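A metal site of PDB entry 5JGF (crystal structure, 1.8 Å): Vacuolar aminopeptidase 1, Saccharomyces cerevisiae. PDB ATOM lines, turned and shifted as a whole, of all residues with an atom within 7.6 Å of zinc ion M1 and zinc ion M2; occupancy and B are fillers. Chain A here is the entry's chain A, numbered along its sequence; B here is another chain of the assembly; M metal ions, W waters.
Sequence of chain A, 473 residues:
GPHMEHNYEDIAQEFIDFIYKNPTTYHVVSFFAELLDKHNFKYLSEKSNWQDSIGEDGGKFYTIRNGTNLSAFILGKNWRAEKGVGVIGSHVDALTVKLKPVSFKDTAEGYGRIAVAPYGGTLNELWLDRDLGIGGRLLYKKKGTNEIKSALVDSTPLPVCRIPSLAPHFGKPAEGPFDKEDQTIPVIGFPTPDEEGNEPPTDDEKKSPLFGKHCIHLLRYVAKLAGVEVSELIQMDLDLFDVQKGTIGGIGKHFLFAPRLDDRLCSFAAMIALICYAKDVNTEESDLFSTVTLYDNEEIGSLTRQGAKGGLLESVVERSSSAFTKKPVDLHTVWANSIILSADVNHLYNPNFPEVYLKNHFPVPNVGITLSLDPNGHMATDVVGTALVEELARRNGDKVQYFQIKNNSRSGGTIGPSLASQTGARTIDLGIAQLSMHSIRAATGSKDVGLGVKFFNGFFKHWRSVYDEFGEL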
ATOM      1  N   SER A  90     -31.399  -8.530 -14.853  1.00  0.00           N
ATOM      2  CA  SER A  90     -30.133  -8.333 -15.552  1.00  0.00           C
ATOM      3  C   SER A  90     -29.476  -7.071 -15.011  1.00  0.00           C
ATOM      4  O   SER A  90     -30.088  -6.326 -14.242  1.00  0.00           O
ATOM      5  CB  SER A  90     -30.364  -8.163 -17.058  1.00  0.00           C
ATOM      6  OG  SER A  90     -30.980  -9.308 -17.625  1.00  0.00           O
ATOM      7  N   HIS A  91     -28.221  -6.820 -15.384  1.00  0.00           N
ATOM      8  CA  HIS A  91     -27.571  -5.599 -14.913  1.00  0.00           C
ATOM      9  C   HIS A  91     -27.235  -4.672 -16.073  1.00  0.00           C
ATOM     10  O   HIS A  91     -26.902  -5.114 -17.172  1.00  0.00           O
ATOM     11  CB  HIS A  91     -26.342  -5.910 -14.031  1.00  0.00           C
ATOM     12  CG  HIS A  91     -25.170  -6.522 -14.742  1.00  0.00           C
ATOM     13  ND1 HIS A  91     -24.172  -5.765 -15.323  1.00  0.00           N
ATOM     14  CD2 HIS A  91     -24.796  -7.818 -14.870  1.00  0.00           C
ATOM     15  CE1 HIS A  91     -23.233  -6.575 -15.774  1.00  0.00           C
ATOM     16  NE2 HIS A  91     -23.584  -7.824 -15.516  1.00  0.00           N
ATOM     17  N   ASP A  93     -25.071  -1.892 -15.589  1.00  0.00           N
ATOM     18  CA  ASP A  93     -23.779  -1.257 -15.416  1.00  0.00           C
ATOM     19  C   ASP A  93     -22.775  -2.102 -16.193  1.00  0.00           C
ATOM     20  O   ASP A  93     -22.980  -3.299 -16.376  1.00  0.00           O
ATOM     21  CB  ASP A  93     -23.367  -1.179 -13.938  1.00  0.00           C
ATOM     22  CG  ASP A  93     -23.168  -2.548 -13.305  1.00  0.00           C
ATOM     23  OD1 ASP A  93     -22.130  -2.742 -12.641  1.00  0.00           O
ATOM     24  OD2 ASP A  93     -24.063  -3.409 -13.436  1.00  0.00           O
ATOM     25  N   ALA A  94     -21.725  -1.473 -16.685  1.00  0.00           N
ATOM     26  CA  ALA A  94     -20.693  -2.192 -17.426  1.00  0.00           C
ATOM     27  C   ALA A  94     -19.345  -1.616 -17.022  1.00  0.00           C
ATOM     28  O   ALA A  94     -19.266  -0.480 -16.558  1.00  0.00           O
ATOM     29  CB  ALA A  94     -20.909  -2.004 -18.928  1.00  0.00           C
ATOM     30  N   LEU A  95     -18.288  -2.412 -17.168  1.00  0.00           N
ATOM     31  CA  LEU A  95     -16.966  -1.927 -16.827  1.00  0.00           C
ATOM     32  C   LEU A  95     -16.721  -0.612 -17.545  1.00  0.00           C
ATOM     33  O   LEU A  95     -17.025  -0.484 -18.738  1.00  0.00           O
ATOM     34  CB  LEU A  95     -15.891  -2.943 -17.236  1.00  0.00           C
ATOM     35  CG  LEU A  95     -15.362  -3.844 -16.112  1.00  0.00           C
ATOM     36  CD1 LEU A  95     -16.514  -4.596 -15.465  1.00  0.00           C
ATOM     37  CD2 LEU A  95     -14.322  -4.799 -16.681  1.00  0.00           C
ATOM     38  N   LEU A 261     -20.951  -5.231 -23.847  1.00  0.00           N
ATOM     39  CA  LEU A 261     -21.952  -6.291 -24.046  1.00  0.00           C
ATOM     40  C   LEU A 261     -22.435  -6.846 -22.693  1.00  0.00           C
ATOM     41  O   LEU A 261     -23.604  -7.158 -22.527  1.00  0.00           O
ATOM     42  CB  LEU A 261     -21.360  -7.427 -24.896  1.00  0.00           C
ATOM     43  CG  LEU A 261     -21.032  -7.142 -26.361  1.00  0.00           C
ATOM     44  CD1 LEU A 261     -20.672  -8.454 -27.073  1.00  0.00           C
ATOM     45  CD2 LEU A 261     -22.241  -6.506 -27.041  1.00  0.00           C
ATOM     46  N   ASP A 262     -21.516  -6.975 -21.751  1.00  0.00           N
ATOM     47  CA  ASP A 262     -21.834  -7.466 -20.418  1.00  0.00           C
ATOM     48  C   ASP A 262     -22.294  -6.277 -19.551  1.00  0.00           C
ATOM     49  O   ASP A 262     -21.493  -5.397 -19.253  1.00  0.00           O
ATOM     50  CB  ASP A 262     -20.543  -8.077 -19.810  1.00  0.00           C
ATOM     51  CG  ASP A 262     -20.712  -8.568 -18.381  1.00  0.00           C
ATOM     52  OD1 ASP A 262     -21.853  -8.623 -17.900  1.00  0.00           O
ATOM     53  OD2 ASP A 262     -19.711  -8.924 -17.720  1.00  0.00           O
ATOM     54  N   ASP A 263     -23.583  -6.172 -19.190  1.00  0.00           N
ATOM     55  CA  ASP A 263     -24.638  -7.140 -19.510  1.00  0.00           C
ATOM     56  C   ASP A 263     -25.789  -6.450 -20.276  1.00  0.00           C
ATOM     57  O   ASP A 263     -26.952  -6.820 -20.150  1.00  0.00           O
ATOM     58  CB  ASP A 263     -25.121  -7.776 -18.190  1.00  0.00           C
ATOM     59  CG  ASP A 263     -26.209  -8.825 -18.368  1.00  0.00           C
ATOM     60  OD1 ASP A 263     -26.196  -9.590 -19.358  1.00  0.00           O
ATOM     61  OD2 ASP A 263     -27.101  -8.920 -17.491  1.00  0.00           O
ATOM     62  N   ARG A 264     -25.469  -5.419 -21.067  1.00  0.00           N
ATOM     63  CA  ARG A 264     -26.491  -4.693 -21.803  1.00  0.00           C
ATOM     64  C   ARG A 264     -27.034  -5.538 -22.951  1.00  0.00           C
ATOM     65  O   ARG A 264     -28.077  -5.232 -23.526  1.00  0.00           O
ATOM     66  CB  ARG A 264     -25.915  -3.367 -22.304  1.00  0.00           C
ATOM     67  CG  ARG A 264     -25.712  -2.398 -21.134  1.00  0.00           C
ATOM     68  CD  ARG A 264     -24.795  -1.230 -21.427  1.00  0.00           C
ATOM     69  NE  ARG A 264     -24.511  -0.527 -20.171  1.00  0.00           N
ATOM     70  CZ  ARG A 264     -23.770   0.566 -20.057  1.00  0.00           C
ATOM     71  NH1 ARG A 264     -23.224   1.101 -21.139  1.00  0.00           N
ATOM     72  NH2 ARG A 264     -23.560   1.106 -18.862  1.00  0.00           N
ATOM     73  N   GLU A 298     -23.562  -4.459 -10.572  1.00  0.00           N
ATOM     74  CA  GLU A 298     -23.288  -5.886 -10.481  1.00  0.00           C
ATOM     75  C   GLU A 298     -21.773  -6.109 -10.567  1.00  0.00           C
ATOM     76  O   GLU A 298     -21.219  -7.010  -9.936  1.00  0.00           O
ATOM     77  CB  GLU A 298     -23.990  -6.646 -11.611  1.00  0.00           C
ATOM     78  CG  GLU A 298     -23.833  -8.181 -11.569  1.00  0.00           C
ATOM     79  CD  GLU A 298     -22.453  -8.677 -11.974  1.00  0.00           C
ATOM     80  OE1 GLU A 298     -21.791  -8.016 -12.810  1.00  0.00           O
ATOM     81  OE2 GLU A 298     -22.037  -9.749 -11.478  1.00  0.00           O
ATOM     82  N   GLU A 299     -21.114  -5.260 -11.354  1.00  0.00           N
ATOM     83  CA  GLU A 299     -19.674  -5.373 -11.556  1.00  0.00           C
ATOM     84  C   GLU A 299     -18.857  -5.034 -10.304  1.00  0.00           C
ATOM     85  O   GLU A 299     -17.648  -5.270 -10.286  1.00  0.00           O
ATOM     86  CB  GLU A 299     -19.237  -4.497 -12.737  1.00  0.00           C
ATOM     87  CG  GLU A 299     -19.871  -4.899 -14.085  1.00  0.00           C
ATOM     88  CD  GLU A 299     -19.437  -6.279 -14.575  1.00  0.00           C
ATOM     89  OE1 GLU A 299     -18.800  -7.026 -13.796  1.00  0.00           O
ATOM     90  OE2 GLU A 299     -19.741  -6.625 -15.736  1.00  0.00           O
ATOM     91  N   ALA A 343     -30.521 -13.219 -15.941  1.00  0.00           N
ATOM     92  CA  ALA A 343     -29.891 -13.148 -17.245  1.00  0.00           C
ATOM     93  C   ALA A 343     -28.635 -12.300 -17.278  1.00  0.00           C
ATOM     94  O   ALA A 343     -28.687 -11.075 -17.253  1.00  0.00           O
ATOM     95  CB  ALA A 343     -30.902 -12.624 -18.281  1.00  0.00           C
ATOM     96  N   ASP A 344     -27.495 -12.981 -17.323  1.00  0.00           N
ATOM     97  CA  ASP A 344     -26.203 -12.311 -17.380  1.00  0.00           C
ATOM     98  C   ASP A 344     -25.397 -13.078 -18.415  1.00  0.00           C
ATOM     99  O   ASP A 344     -25.427 -14.305 -18.457  1.00  0.00           O
ATOM    100  CB  ASP A 344     -25.500 -12.364 -16.013  1.00  0.00           C
ATOM    101  CG  ASP A 344     -24.402 -11.318 -15.885  1.00  0.00           C
ATOM    102  OD1 ASP A 344     -24.068 -10.682 -16.918  1.00  0.00           O
ATOM    103  OD2 ASP A 344     -23.882 -11.127 -14.769  1.00  0.00           O
ATOM    104  N   VAL A 345     -24.694 -12.345 -19.278  1.00  0.00           N
ATOM    105  CA  VAL A 345     -23.901 -12.974 -20.323  1.00  0.00           C
ATOM    106  C   VAL A 345     -22.913 -13.988 -19.743  1.00  0.00           C
ATOM    107  O   VAL A 345     -22.392 -13.802 -18.640  1.00  0.00           O
ATOM    108  CB  VAL A 345     -23.120 -11.925 -21.146  1.00  0.00           C
ATOM    109  CG1 VAL A 345     -24.082 -11.013 -21.898  1.00  0.00           C
ATOM    110  CG2 VAL A 345     -22.228 -11.097 -20.221  1.00  0.00           C
ATOM    111  N   ASN A 346     -22.695 -15.081 -20.458  1.00  0.00           N
ATOM    112  CA  ASN A 346     -21.732 -16.079 -20.045  1.00  0.00           C
ATOM    113  C   ASN A 346     -20.693 -16.208 -21.141  1.00  0.00           C
ATOM    114  O   ASN A 346     -20.711 -15.435 -22.105  1.00  0.00           O
ATOM    115  CB  ASN A 346     -22.384 -17.435 -19.726  1.00  0.00           C
ATOM    116  CG  ASN A 346     -23.613 -17.700 -20.549  1.00  0.00           C
ATOM    117  OD1 ASN A 346     -23.627 -17.482 -21.754  1.00  0.00           O
ATOM    118  ND2 ASN A 346     -24.668 -18.204 -19.904  1.00  0.00           N
ATOM    119  N   GLY A 413     -19.226 -14.400 -11.085  1.00  0.00           N
ATOM    120  CA  GLY A 413     -20.451 -14.407 -10.315  1.00  0.00           C
ATOM    121  C   GLY A 413     -21.577 -13.666 -11.003  1.00  0.00           C
ATOM    122  O   GLY A 413     -21.372 -13.047 -12.049  1.00  0.00           O
ATOM    123  N   THR A 414     -22.765 -13.722 -10.423  1.00  0.00           N
ATOM    124  CA  THR A 414     -23.929 -13.031 -10.972  1.00  0.00           C
ATOM    125  C   THR A 414     -24.825 -12.619  -9.807  1.00  0.00           C
ATOM    126  O   THR A 414     -24.518 -12.895  -8.647  1.00  0.00           O
ATOM    127  CB  THR A 414     -24.767 -13.942 -11.898  1.00  0.00           C
ATOM    128  OG1 THR A 414     -25.427 -14.934 -11.100  1.00  0.00           O
ATOM    129  CG2 THR A 414     -23.890 -14.618 -12.938  1.00  0.00           C
ATOM    130  N   ILE A 415     -25.937 -11.956 -10.128  1.00  0.00           N
ATOM    131  CA  ILE A 415     -26.885 -11.538  -9.102  1.00  0.00           C
ATOM    132  C   ILE A 415     -27.841 -12.684  -8.776  1.00  0.00           C
ATOM    133  O   ILE A 415     -28.685 -12.563  -7.882  1.00  0.00           O
ATOM    134  CB  ILE A 415     -27.756 -10.354  -9.587  1.00  0.00           C
ATOM    135  CG1 ILE A 415     -28.579 -10.783 -10.801  1.00  0.00           C
ATOM    136  CG2 ILE A 415     -26.867  -9.152  -9.911  1.00  0.00           C
ATOM    137  CD1 ILE A 415     -29.504  -9.695 -11.337  1.00  0.00           C
ATOM    138  N   GLN A 434     -20.938 -14.703 -24.846  1.00  0.00           N
ATOM    139  CA  GLN A 434     -20.128 -13.755 -25.608  1.00  0.00           C
ATOM    140  C   GLN A 434     -18.646 -14.062 -25.444  1.00  0.00           C
ATOM    141  O   GLN A 434     -18.228 -14.734 -24.503  1.00  0.00           O
ATOM    142  CB  GLN A 434     -20.383 -12.329 -25.108  1.00  0.00           C
ATOM    143  CG  GLN A 434     -19.842 -12.064 -23.705  1.00  0.00           C
ATOM    144  CD  GLN A 434     -19.775 -10.584 -23.366  1.00  0.00           C
ATOM    145  OE1 GLN A 434     -20.735 -10.007 -22.854  1.00  0.00           O
ATOM    146  NE2 GLN A 434     -18.638  -9.974 -23.666  1.00  0.00           N
ATOM    147  N   MET A 437     -15.403 -11.302 -22.601  1.00  0.00           N
ATOM    148  CA  MET A 437     -16.154 -10.600 -21.582  1.00  0.00           C
ATOM    149  C   MET A 437     -15.192  -9.690 -20.803  1.00  0.00           C
ATOM    150  O   MET A 437     -14.058 -10.083 -20.509  1.00  0.00           O
ATOM    151  CB  MET A 437     -16.821 -11.600 -20.624  1.00  0.00           C
ATOM    152  CG  MET A 437     -17.941 -11.013 -19.791  1.00  0.00           C
ATOM    153  SD  MET A 437     -18.612 -12.236 -18.646  1.00  0.00           S
ATOM    154  CE  MET A 437     -19.300 -13.422 -19.805  1.00  0.00           C
ATOM    155  N   HIS A 438     -15.645  -8.472 -20.510  1.00  0.00           N
ATOM    156  CA  HIS A 438     -14.894  -7.457 -19.789  1.00  0.00           C
ATOM    157  C   HIS A 438     -13.813  -6.729 -20.581  1.00  0.00           C
ATOM    158  O   HIS A 438     -13.079  -5.904 -20.040  1.00  0.00           O
ATOM    159  CB  HIS A 438     -14.311  -8.019 -18.485  1.00  0.00           C
ATOM    160  CG  HIS A 438     -15.336  -8.234 -17.414  1.00  0.00           C
ATOM    161  ND1 HIS A 438     -15.019  -8.504 -16.103  1.00  0.00           N
ATOM    162  CD2 HIS A 438     -16.692  -8.213 -17.471  1.00  0.00           C
ATOM    163  CE1 HIS A 438     -16.121  -8.638 -15.394  1.00  0.00           C
ATOM    164  NE2 HIS A 438     -17.158  -8.463 -16.195  1.00  0.00           N
ATOM    165  N   HIS B 169     -12.074 -13.681 -16.199  1.00  0.00           N
ATOM    166  CA  HIS B 169     -12.748 -14.579 -15.262  1.00  0.00           C
ATOM    167  C   HIS B 169     -12.025 -15.916 -15.122  1.00  0.00           C
ATOM    168  O   HIS B 169     -12.098 -16.567 -14.078  1.00  0.00           O
ATOM    169  CB  HIS B 169     -14.183 -14.853 -15.742  1.00  0.00           C
ATOM    170  CG  HIS B 169     -15.005 -13.613 -15.923  1.00  0.00           C
ATOM    171  ND1 HIS B 169     -14.675 -12.640 -16.844  1.00  0.00           N
ATOM    172  CD2 HIS B 169     -16.130 -13.188 -15.300  1.00  0.00           C
ATOM    173  CE1 HIS B 169     -15.569 -11.670 -16.779  1.00  0.00           C
ATOM    174  NE2 HIS B 169     -16.462 -11.970 -15.848  1.00  0.00           N
HETATM  175 ZN    ZN M   1     -19.254  -8.579 -15.859  1.00  0.00          ZN
HETATM  176 ZN    ZN M   2     -22.444  -9.537 -16.208  1.00  0.00          ZN
HETATM  177  O   HOH W   1     -20.775  -9.328 -14.859  1.00  0.00           O
HETATM  178  O   HOH W   2     -18.849 -11.219 -14.581  1.00  0.00           O
HETATM  179  O   HOH W   3     -21.451 -11.568 -13.966  1.00  0.00           O
HETATM  180  O   HOH W   4     -21.368 -11.489 -16.842  1.00  0.00           O
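Three residues have an atom within 4 Å of zinc ion M1: Asp 262, Glu 299 and His 438. The nearest printed residue that does not touch zinc ion M1 is Glu 298 (4.01 Å).
Zinc ion M2 is bound by the side-chain carboxylate (OD1) of Asp 262 (2.0 Å), the side-chain carboxylate (OD1) of Asp 344 (2.1 Å), water W1 (2.2 Å), a ring nitrogen (NE2) of His 91 (2.2 Å), water W4 (2.3 Å) and the side-chain carboxylate (OD2) of Asp 344 (2.6 Å).
The backbone carbonyl oxygen of Ala 343 sits close to the side-chain carboxylate of Asp 263. N of Glu 299 sits at hydrogen-bond distance from OD1 of Asp 93 (3.0 Å). N of Glu 298 is in hydrogen-bond range of OD1 of Asp 93, at 3.0 Å. OD1 of Asp 263 sits at hydrogen-bond distance from N of Val 345, 3.1 Å away. The backbone carbonyl oxygen of Asp 93 is in hydrogen-bond range of a ring nitrogen (ND1) of His 91 (2.9 Å). NE2 of His 91 sits close to OE1 of Glu 298 (3.3 Å). N of His 91 lies within hydrogen-bond range of OD2 of Asp 263. The backbone NH (N) of Asp 262 is in hydrogen-bond range of the side-chain amide oxygen (OE1) of Gln 434.
Zinc ion M1 is bound by OD2 of Asp 262 (1.9 Å), water W1 (2.0 Å), OE2 of Glu 299 (2.0 Å) and NE2 of His 438 (2.1 Å). Slightly farther from zinc ion M1 lies the side-chain carboxylate (OE1) of Glu 299 (2.6 Å).
Water W1 bridges the side-chain carboxylate of Glu 298 (2.6 Å) and the side-chain carboxylate of Glu 299 (3.2 Å). Water W4 bridges the backbone carbonyl oxygen of Val 345 and the side-chain sulfur of Met 437. Water W3 lies within hydrogen-bond range of O of Gly 413 (2.4 Å) and OE2 of Glu 298 (3.1 Å).
Asp 263 touches zinc ion M2. Glu 298 touches zinc ion M2 (OE1 to ZN, 3.8 Å). The nearest printed residue that does not touch zinc ion M2 is Glu 299 (4.001 Å).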
